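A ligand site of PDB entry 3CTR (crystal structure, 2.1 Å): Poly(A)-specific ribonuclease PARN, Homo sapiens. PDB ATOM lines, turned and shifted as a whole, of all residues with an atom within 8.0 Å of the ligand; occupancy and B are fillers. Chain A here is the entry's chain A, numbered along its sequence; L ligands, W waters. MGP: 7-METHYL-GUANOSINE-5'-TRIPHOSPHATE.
The backbone NH (N) of Thr 40 lies within hydrogen-bond range of the side-chain carboxylate (OD1) of Asp 38, 3.0 Å away. OD1 of Asp 38 is in hydrogen-bond range of OG of Ser 41 (3.1 Å). The side-chain amino group of Lys 18 sits at hydrogen-bond distance from the backbone carbonyl oxygen of Glu 16, at 3.3 Å. OD2 of Asp 21 sits at hydrogen-bond distance from N of Lys 18, 2.8 Å away.
Merely in contact with the ligand: Asp 38, Lys 18 and Thr 19. Within 4 Å of the ligand: Lys 15, Trp 17, Lys 18, Thr 19, Trp 36, Asp 38 and Asp 39. The nearest printed residue that does not touch the ligand is Ile 34 (4.04 Å).
The backbone carbonyl oxygen of Trp 17 is in hydrogen-bond range of a nitrogen (N1) of the ligand, 2.7 Å away. An oxygen (O2') of the ligand is in hydrogen-bond range of the backbone NH (N) of Asp 39 (3.3 Å). The backbone carbonyl oxygen (O) of Asp 39 sits at hydrogen-bond distance from a nitrogen (N2) of the ligand (2.7 Å). OD1 of Asp 39 is in hydrogen-bond range of O2' of the ligand (2.8 Å). N2 of the ligand lies within hydrogen-bond range of O of Lys 15, 3.0 Å away. O1C of the ligand lies close to NE1 of Trp 36 (3.5 Å).
Water W1 bridges the side-chain hydroxyl of Thr 19 (2.6 Å) and an oxygen (O6) of the ligand (3.4 Å).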
ATOM      1  N   PHE A  13     -21.218 -20.460  -5.332  1.00  0.00           N
ATOM      2  CA  PHE A  13     -22.621 -20.568  -5.697  1.00  0.00           C
ATOM      3  C   PHE A  13     -22.814 -20.337  -7.192  1.00  0.00           C
ATOM      4  O   PHE A  13     -21.879 -19.898  -7.852  1.00  0.00           O
ATOM      5  CB  PHE A  13     -23.438 -19.536  -4.916  1.00  0.00           C
ATOM      6  CG  PHE A  13     -22.754 -18.199  -4.788  1.00  0.00           C
ATOM      7  CD1 PHE A  13     -22.043 -17.886  -3.647  1.00  0.00           C
ATOM      8  CD2 PHE A  13     -22.852 -17.250  -5.814  1.00  0.00           C
ATOM      9  CE1 PHE A  13     -21.420 -16.653  -3.521  1.00  0.00           C
ATOM     10  CE2 PHE A  13     -22.228 -16.021  -5.696  1.00  0.00           C
ATOM     11  CZ  PHE A  13     -21.505 -15.719  -4.540  1.00  0.00           C
ATOM     12  N   PRO A  14     -24.019 -20.613  -7.723  1.00  0.00           N
ATOM     13  CA  PRO A  14     -24.256 -20.292  -9.148  1.00  0.00           C
ATOM     14  C   PRO A  14     -24.263 -18.783  -9.457  1.00  0.00           C
ATOM     15  O   PRO A  14     -24.646 -17.963  -8.602  1.00  0.00           O
ATOM     16  CB  PRO A  14     -25.656 -20.887  -9.416  1.00  0.00           C
ATOM     17  CG  PRO A  14     -25.920 -21.848  -8.272  1.00  0.00           C
ATOM     18  CD  PRO A  14     -25.203 -21.231  -7.099  1.00  0.00           C
ATOM     19  N   LYS A  15     -23.887 -18.428 -10.674  1.00  0.00           N
ATOM     20  CA  LYS A  15     -23.834 -17.021 -11.080  1.00  0.00           C
ATOM     21  C   LYS A  15     -25.176 -16.294 -10.956  1.00  0.00           C
ATOM     22  O   LYS A  15     -25.209 -15.070 -10.806  1.00  0.00           O
ATOM     23  CB  LYS A  15     -23.265 -16.887 -12.510  1.00  0.00           C
ATOM     24  CG  LYS A  15     -24.043 -17.636 -13.588  1.00  0.00           C
ATOM     25  CD  LYS A  15     -23.490 -17.336 -14.982  1.00  0.00           C
ATOM     26  CE  LYS A  15     -24.385 -17.963 -16.062  1.00  0.00           C
ATOM     27  NZ  LYS A  15     -23.594 -18.282 -17.288  1.00  0.00           N
ATOM     28  N   GLU A  16     -26.267 -17.063 -10.983  1.00  0.00           N
ATOM     29  CA  GLU A  16     -27.629 -16.541 -10.917  1.00  0.00           C
ATOM     30  C   GLU A  16     -28.033 -16.011  -9.525  1.00  0.00           C
ATOM     31  O   GLU A  16     -29.032 -15.285  -9.389  1.00  0.00           O
ATOM     32  CB  GLU A  16     -28.620 -17.636 -11.351  1.00  0.00           C
ATOM     33  CG  GLU A  16     -28.604 -17.976 -12.859  1.00  0.00           C
ATOM     34  CD  GLU A  16     -27.442 -18.865 -13.274  1.00  0.00           C
ATOM     35  OE1 GLU A  16     -26.913 -19.623 -12.433  1.00  0.00           O
ATOM     36  OE2 GLU A  16     -27.069 -18.822 -14.477  1.00  0.00           O
ATOM     37  N   TRP A  17     -27.290 -16.390  -8.499  1.00  0.00           N
ATOM     38  CA  TRP A  17     -27.571 -15.946  -7.128  1.00  0.00           C
ATOM     39  C   TRP A  17     -27.387 -14.452  -6.955  1.00  0.00           C
ATOM     40  O   TRP A  17     -26.503 -13.854  -7.591  1.00  0.00           O
ATOM     41  CB  TRP A  17     -26.659 -16.696  -6.146  1.00  0.00           C
ATOM     42  CG  TRP A  17     -27.143 -18.067  -5.753  1.00  0.00           C
ATOM     43  CD1 TRP A  17     -27.912 -18.922  -6.495  1.00  0.00           C
ATOM     44  CD2 TRP A  17     -26.882 -18.746  -4.508  1.00  0.00           C
ATOM     45  NE1 TRP A  17     -28.151 -20.081  -5.791  1.00  0.00           N
ATOM     46  CE2 TRP A  17     -27.516 -20.003  -4.574  1.00  0.00           C
ATOM     47  CE3 TRP A  17     -26.178 -18.403  -3.347  1.00  0.00           C
ATOM     48  CZ2 TRP A  17     -27.470 -20.926  -3.520  1.00  0.00           C
ATOM     49  CZ3 TRP A  17     -26.117 -19.331  -2.300  1.00  0.00           C
ATOM     50  CH2 TRP A  17     -26.759 -20.566  -2.395  1.00  0.00           C
ATOM     51  N   LYS A  18     -28.215 -13.863  -6.105  1.00  0.00           N
ATOM     52  CA  LYS A  18     -28.132 -12.456  -5.719  1.00  0.00           C
ATOM     53  C   LYS A  18     -27.867 -12.325  -4.217  1.00  0.00           C
ATOM     54  O   LYS A  18     -27.755 -13.328  -3.501  1.00  0.00           O
ATOM     55  CB  LYS A  18     -29.441 -11.719  -6.043  1.00  0.00           C
ATOM     56  CG  LYS A  18     -29.926 -11.785  -7.515  1.00  0.00           C
ATOM     57  CD  LYS A  18     -28.992 -11.020  -8.460  1.00  0.00           C
ATOM     58  CE  LYS A  18     -29.567 -10.920  -9.883  1.00  0.00           C
ATOM     59  NZ  LYS A  18     -29.639 -12.254 -10.559  1.00  0.00           N
ATOM     60  N   THR A  19     -27.761 -11.082  -3.750  1.00  0.00           N
ATOM     61  CA  THR A  19     -27.595 -10.770  -2.332  1.00  0.00           C
ATOM     62  C   THR A  19     -28.618 -11.518  -1.465  1.00  0.00           C
ATOM     63  O   THR A  19     -28.267 -12.100  -0.449  1.00  0.00           O
ATOM     64  CB  THR A  19     -27.748  -9.247  -2.085  1.00  0.00           C
ATOM     65  OG1 THR A  19     -26.922  -8.536  -3.012  1.00  0.00           O
ATOM     66  CG2 THR A  19     -27.319  -8.884  -0.670  1.00  0.00           C
ATOM     67  N   SER A  20     -29.878 -11.512  -1.899  1.00  0.00           N
ATOM     68  CA  SER A  20     -30.983 -12.070  -1.129  1.00  0.00           C
ATOM     69  C   SER A  20     -30.814 -13.557  -0.886  1.00  0.00           C
ATOM     70  O   SER A  20     -31.174 -14.019   0.178  1.00  0.00           O
ATOM     71  CB  SER A  20     -32.320 -11.818  -1.828  1.00  0.00           C
ATOM     72  OG  SER A  20     -32.226 -12.244  -3.180  1.00  0.00           O
ATOM     73  N   ASP A  21     -30.285 -14.296  -1.863  1.00  0.00           N
ATOM     74  CA  ASP A  21     -30.012 -15.722  -1.706  1.00  0.00           C
ATOM     75  C   ASP A  21     -29.011 -15.990  -0.598  1.00  0.00           C
ATOM     76  O   ASP A  21     -29.182 -16.916   0.202  1.00  0.00           O
ATOM     77  CB  ASP A  21     -29.512 -16.326  -3.009  1.00  0.00           C
ATOM     78  CG  ASP A  21     -30.540 -16.240  -4.109  1.00  0.00           C
ATOM     79  OD1 ASP A  21     -31.576 -16.919  -4.002  1.00  0.00           O
ATOM     80  OD2 ASP A  21     -30.307 -15.466  -5.062  1.00  0.00           O
ATOM     81  N   LEU A  22     -27.971 -15.176  -0.528  1.00  0.00           N
ATOM     82  CA  LEU A  22     -26.952 -15.365   0.511  1.00  0.00           C
ATOM     83  C   LEU A  22     -27.519 -14.976   1.884  1.00  0.00           C
ATOM     84  O   LEU A  22     -27.260 -15.678   2.860  1.00  0.00           O
ATOM     85  CB  LEU A  22     -25.684 -14.588   0.191  1.00  0.00           C
ATOM     86  CG  LEU A  22     -24.783 -15.147  -0.919  1.00  0.00           C
ATOM     87  CD1 LEU A  22     -23.658 -14.125  -1.223  1.00  0.00           C
ATOM     88  CD2 LEU A  22     -24.168 -16.490  -0.524  1.00  0.00           C
ATOM     89  N   TYR A  23     -28.284 -13.889   1.938  1.00  0.00           N
ATOM     90  CA  TYR A  23     -29.011 -13.503   3.168  1.00  0.00           C
ATOM     91  C   TYR A  23     -29.955 -14.625   3.653  1.00  0.00           C
ATOM     92  O   TYR A  23     -30.009 -14.928   4.851  1.00  0.00           O
ATOM     93  CB  TYR A  23     -29.806 -12.199   2.961  1.00  0.00           C
ATOM     94  CG  TYR A  23     -28.963 -10.929   2.978  1.00  0.00           C
ATOM     95  CD1 TYR A  23     -27.686 -10.918   3.515  1.00  0.00           C
ATOM     96  CD2 TYR A  23     -29.470  -9.723   2.472  1.00  0.00           C
ATOM     97  CE1 TYR A  23     -26.908  -9.760   3.555  1.00  0.00           C
ATOM     98  CE2 TYR A  23     -28.680  -8.532   2.501  1.00  0.00           C
ATOM     99  CZ  TYR A  23     -27.404  -8.585   3.049  1.00  0.00           C
ATOM    100  OH  TYR A  23     -26.596  -7.459   3.115  1.00  0.00           O
ATOM    101  N   GLN A  33     -22.592  -9.937   6.381  1.00  0.00           N
ATOM    102  CA  GLN A  33     -21.960  -8.995   5.471  1.00  0.00           C
ATOM    103  C   GLN A  33     -21.318  -9.800   4.349  1.00  0.00           C
ATOM    104  O   GLN A  33     -20.539 -10.724   4.580  1.00  0.00           O
ATOM    105  CB  GLN A  33     -20.971  -8.081   6.215  1.00  0.00           C
ATOM    106  CG  GLN A  33     -21.666  -7.261   7.316  1.00  0.00           C
ATOM    107  CD  GLN A  33     -20.734  -6.413   8.173  1.00  0.00           C
ATOM    108  OE1 GLN A  33     -20.289  -6.837   9.250  1.00  0.00           O
ATOM    109  NE2 GLN A  33     -20.466  -5.204   7.720  1.00  0.00           N
ATOM    110  N   ILE A  34     -21.698  -9.478   3.133  1.00  0.00           N
ATOM    111  CA  ILE A  34     -21.168 -10.177   1.962  1.00  0.00           C
ATOM    112  C   ILE A  34     -19.991  -9.391   1.363  1.00  0.00           C
ATOM    113  O   ILE A  34     -20.116  -8.203   1.102  1.00  0.00           O
ATOM    114  CB  ILE A  34     -22.266 -10.376   0.903  1.00  0.00           C
ATOM    115  CG1 ILE A  34     -23.405 -11.233   1.488  1.00  0.00           C
ATOM    116  CG2 ILE A  34     -21.690 -10.995  -0.388  1.00  0.00           C
ATOM    117  CD1 ILE A  34     -24.740 -10.952   0.854  1.00  0.00           C
ATOM    118  N   SER A  35     -18.850 -10.050   1.175  1.00  0.00           N
ATOM    119  CA  SER A  35     -17.719  -9.446   0.465  1.00  0.00           C
ATOM    120  C   SER A  35     -17.539 -10.202  -0.870  1.00  0.00           C
ATOM    121  O   SER A  35     -16.954 -11.261  -0.897  1.00  0.00           O
ATOM    122  CB  SER A  35     -16.465  -9.518   1.326  1.00  0.00           C
ATOM    123  OG  SER A  35     -16.601  -8.737   2.507  1.00  0.00           O
ATOM    124  N   TRP A  36     -18.127  -9.704  -1.944  1.00  0.00           N
ATOM    125  CA  TRP A  36     -18.071 -10.419  -3.230  1.00  0.00           C
ATOM    126  C   TRP A  36     -16.663 -10.561  -3.735  1.00  0.00           C
ATOM    127  O   TRP A  36     -15.879  -9.618  -3.640  1.00  0.00           O
ATOM    128  CB  TRP A  36     -18.906  -9.702  -4.278  1.00  0.00           C
ATOM    129  CG  TRP A  36     -20.333  -9.543  -3.888  1.00  0.00           C
ATOM    130  CD1 TRP A  36     -20.895  -8.468  -3.268  1.00  0.00           C
ATOM    131  CD2 TRP A  36     -21.391 -10.470  -4.122  1.00  0.00           C
ATOM    132  NE1 TRP A  36     -22.234  -8.663  -3.106  1.00  0.00           N
ATOM    133  CE2 TRP A  36     -22.576  -9.885  -3.613  1.00  0.00           C
ATOM    134  CE3 TRP A  36     -21.465 -11.748  -4.701  1.00  0.00           C
ATOM    135  CZ2 TRP A  36     -23.819 -10.538  -3.653  1.00  0.00           C
ATOM    136  CZ3 TRP A  36     -22.697 -12.386  -4.756  1.00  0.00           C
ATOM    137  CH2 TRP A  36     -23.854 -11.780  -4.220  1.00  0.00           C
ATOM    138  N   ILE A  37     -16.326 -11.760  -4.216  1.00  0.00           N
ATOM    139  CA  ILE A  37     -15.044 -12.076  -4.821  1.00  0.00           C
ATOM    140  C   ILE A  37     -15.177 -12.021  -6.365  1.00  0.00           C
ATOM    141  O   ILE A  37     -14.428 -11.302  -7.036  1.00  0.00           O
ATOM    142  CB  ILE A  37     -14.521 -13.464  -4.355  1.00  0.00           C
ATOM    143  CG1 ILE A  37     -14.119 -13.420  -2.873  1.00  0.00           C
ATOM    144  CG2 ILE A  37     -13.354 -13.942  -5.244  1.00  0.00           C
ATOM    145  CD1 ILE A  37     -13.989 -14.765  -2.226  1.00  0.00           C
ATOM    146  N   ASP A  38     -16.142 -12.770  -6.898  1.00  0.00           N
ATOM    147  CA  ASP A  38     -16.423 -12.762  -8.334  1.00  0.00           C
ATOM    148  C   ASP A  38     -17.861 -13.230  -8.554  1.00  0.00           C
ATOM    149  O   ASP A  38     -18.689 -13.131  -7.637  1.00  0.00           O
ATOM    150  CB  ASP A  38     -15.407 -13.606  -9.119  1.00  0.00           C
ATOM    151  CG  ASP A  38     -15.337 -15.060  -8.643  1.00  0.00           C
ATOM    152  OD1 ASP A  38     -16.362 -15.594  -8.192  1.00  0.00           O
ATOM    153  OD2 ASP A  38     -14.256 -15.664  -8.718  1.00  0.00           O
ATOM    154  N   ASP A  39     -18.173 -13.719  -9.754  1.00  0.00           N
ATOM    155  CA  ASP A  39     -19.552 -14.030 -10.130  1.00  0.00           C
ATOM    156  C   ASP A  39     -20.134 -15.176  -9.314  1.00  0.00           C
ATOM    157  O   ASP A  39     -21.340 -15.248  -9.087  1.00  0.00           O
ATOM    158  CB  ASP A  39     -19.661 -14.384 -11.624  1.00  0.00           C
ATOM    159  CG  ASP A  39     -19.893 -13.160 -12.515  1.00  0.00           C
ATOM    160  OD1 ASP A  39     -19.810 -12.009 -11.997  1.00  0.00           O
ATOM    161  OD2 ASP A  39     -20.151 -13.355 -13.738  1.00  0.00           O
ATOM    162  N   THR A  40     -19.263 -16.082  -8.899  1.00  0.00           N
ATOM    163  CA  THR A  40     -19.690 -17.334  -8.308  1.00  0.00           C
ATOM    164  C   THR A  40     -19.063 -17.566  -6.941  1.00  0.00           C
ATOM    165  O   THR A  40     -18.984 -18.705  -6.510  1.00  0.00           O
ATOM    166  CB  THR A  40     -19.326 -18.524  -9.195  1.00  0.00           C
ATOM    167  OG1 THR A  40     -17.905 -18.572  -9.348  1.00  0.00           O
ATOM    168  CG2 THR A  40     -20.008 -18.441 -10.579  1.00  0.00           C
ATOM    169  N   SER A  41     -18.610 -16.504  -6.259  1.00  0.00           N
ATOM    170  CA  SER A  41     -18.037 -16.653  -4.915  1.00  0.00           C
ATOM    171  C   SER A  41     -17.968 -15.338  -4.116  1.00  0.00           C
ATOM    172  O   SER A  41     -17.946 -14.246  -4.690  1.00  0.00           O
ATOM    173  CB  SER A  41     -16.696 -17.388  -4.930  1.00  0.00           C
ATOM    174  OG  SER A  41     -15.620 -16.574  -5.400  1.00  0.00           O
ATOM    175  N   ALA A  42     -17.958 -15.477  -2.788  1.00  0.00           N
ATOM    176  CA  ALA A  42     -17.996 -14.344  -1.860  1.00  0.00           C
ATOM    177  C   ALA A  42     -17.461 -14.814  -0.524  1.00  0.00           C
ATOM    178  O   ALA A  42     -17.527 -16.007  -0.227  1.00  0.00           O
ATOM    179  CB  ALA A  42     -19.421 -13.834  -1.700  1.00  0.00           C
HETATM  180  PA  MGP L   1     -20.288  -4.874  -7.106  1.00  0.00           P
HETATM  181  O1A MGP L   1     -21.583  -5.131  -7.801  1.00  0.00           O
HETATM  182  O2A MGP L   1     -19.331  -3.888  -7.679  1.00  0.00           O
HETATM  183  O3A MGP L   1     -20.632  -4.496  -5.579  1.00  0.00           O
HETATM  184  O5' MGP L   1     -19.535  -6.308  -6.899  1.00  0.00           O
HETATM  185  PB  MGP L   1     -19.478  -4.444  -4.463  1.00  0.00           P
HETATM  186  O1B MGP L   1     -18.381  -3.574  -4.939  1.00  0.00           O
HETATM  187  O2B MGP L   1     -19.175  -5.830  -4.019  1.00  0.00           O
HETATM  188  O3B MGP L   1     -20.255  -3.680  -3.275  1.00  0.00           O
HETATM  189  PC  MGP L   1     -21.513  -4.337  -2.506  1.00  0.00           P
HETATM  190  O1C MGP L   1     -21.205  -5.600  -1.785  1.00  0.00           O
HETATM  191  O2C MGP L   1     -22.723  -4.521  -3.570  1.00  0.00           O
HETATM  192  O3C MGP L   1     -21.995  -3.164  -1.497  1.00  0.00           O
HETATM  193  C5' MGP L   1     -18.357  -6.662  -7.618  1.00  0.00           C
HETATM  194  C4' MGP L   1     -18.420  -8.099  -8.171  1.00  0.00           C
HETATM  195  O4' MGP L   1     -19.061  -9.023  -7.237  1.00  0.00           O
HETATM  196  C3' MGP L   1     -19.280  -8.140  -9.444  1.00  0.00           C
HETATM  197  O3' MGP L   1     -18.440  -7.849 -10.583  1.00  0.00           O
HETATM  198  C2' MGP L   1     -19.740  -9.602  -9.463  1.00  0.00           C
HETATM  199  O2' MGP L   1     -18.705 -10.434 -10.006  1.00  0.00           O
HETATM  200  C1' MGP L   1     -19.929  -9.929  -7.971  1.00  0.00           C
HETATM  201  N9  MGP L   1     -21.319  -9.660  -7.552  1.00  0.00           N
HETATM  202  C8  MGP L   1     -21.793  -8.546  -6.980  1.00  0.00           C
HETATM  203  N7  MGP L   1     -23.096  -8.694  -6.778  1.00  0.00           N
HETATM  204  CM7 MGP L   1     -23.927  -7.646  -6.153  1.00  0.00           C
HETATM  205  C5  MGP L   1     -23.489  -9.899  -7.211  1.00  0.00           C
HETATM  206  C6  MGP L   1     -24.710 -10.599  -7.243  1.00  0.00           C
HETATM  207  O6  MGP L   1     -25.753 -10.133  -6.807  1.00  0.00           O
HETATM  208  N1  MGP L   1     -24.708 -11.888  -7.800  1.00  0.00           N
HETATM  209  C2  MGP L   1     -23.515 -12.428  -8.282  1.00  0.00           C
HETATM  210  N2  MGP L   1     -23.482 -13.650  -8.806  1.00  0.00           N
HETATM  211  N3  MGP L   1     -22.376 -11.734  -8.234  1.00  0.00           N
HETATM  212  C4  MGP L   1     -22.338 -10.505  -7.705  1.00  0.00           C
HETATM  213  O   HOH W   1     -28.172  -8.183  -5.313  1.00  0.00           O
HETATM  214  O   HOH W   2     -23.191  -7.541  -9.824  1.00  0.00           O
HETATM  215  O   HOH W   3     -20.044  -4.511 -10.606  1.00  0.00           O
HETATM  216  O   HOH W   4     -26.040  -9.987 -10.304  1.00  0.00           O
HETATM  217  O   HOH W   5     -17.476  -4.880 -10.300  1.00  0.00           O
HETATM  218  O   HOH W   6     -16.342  -6.323  -5.102  1.00  0.00           O
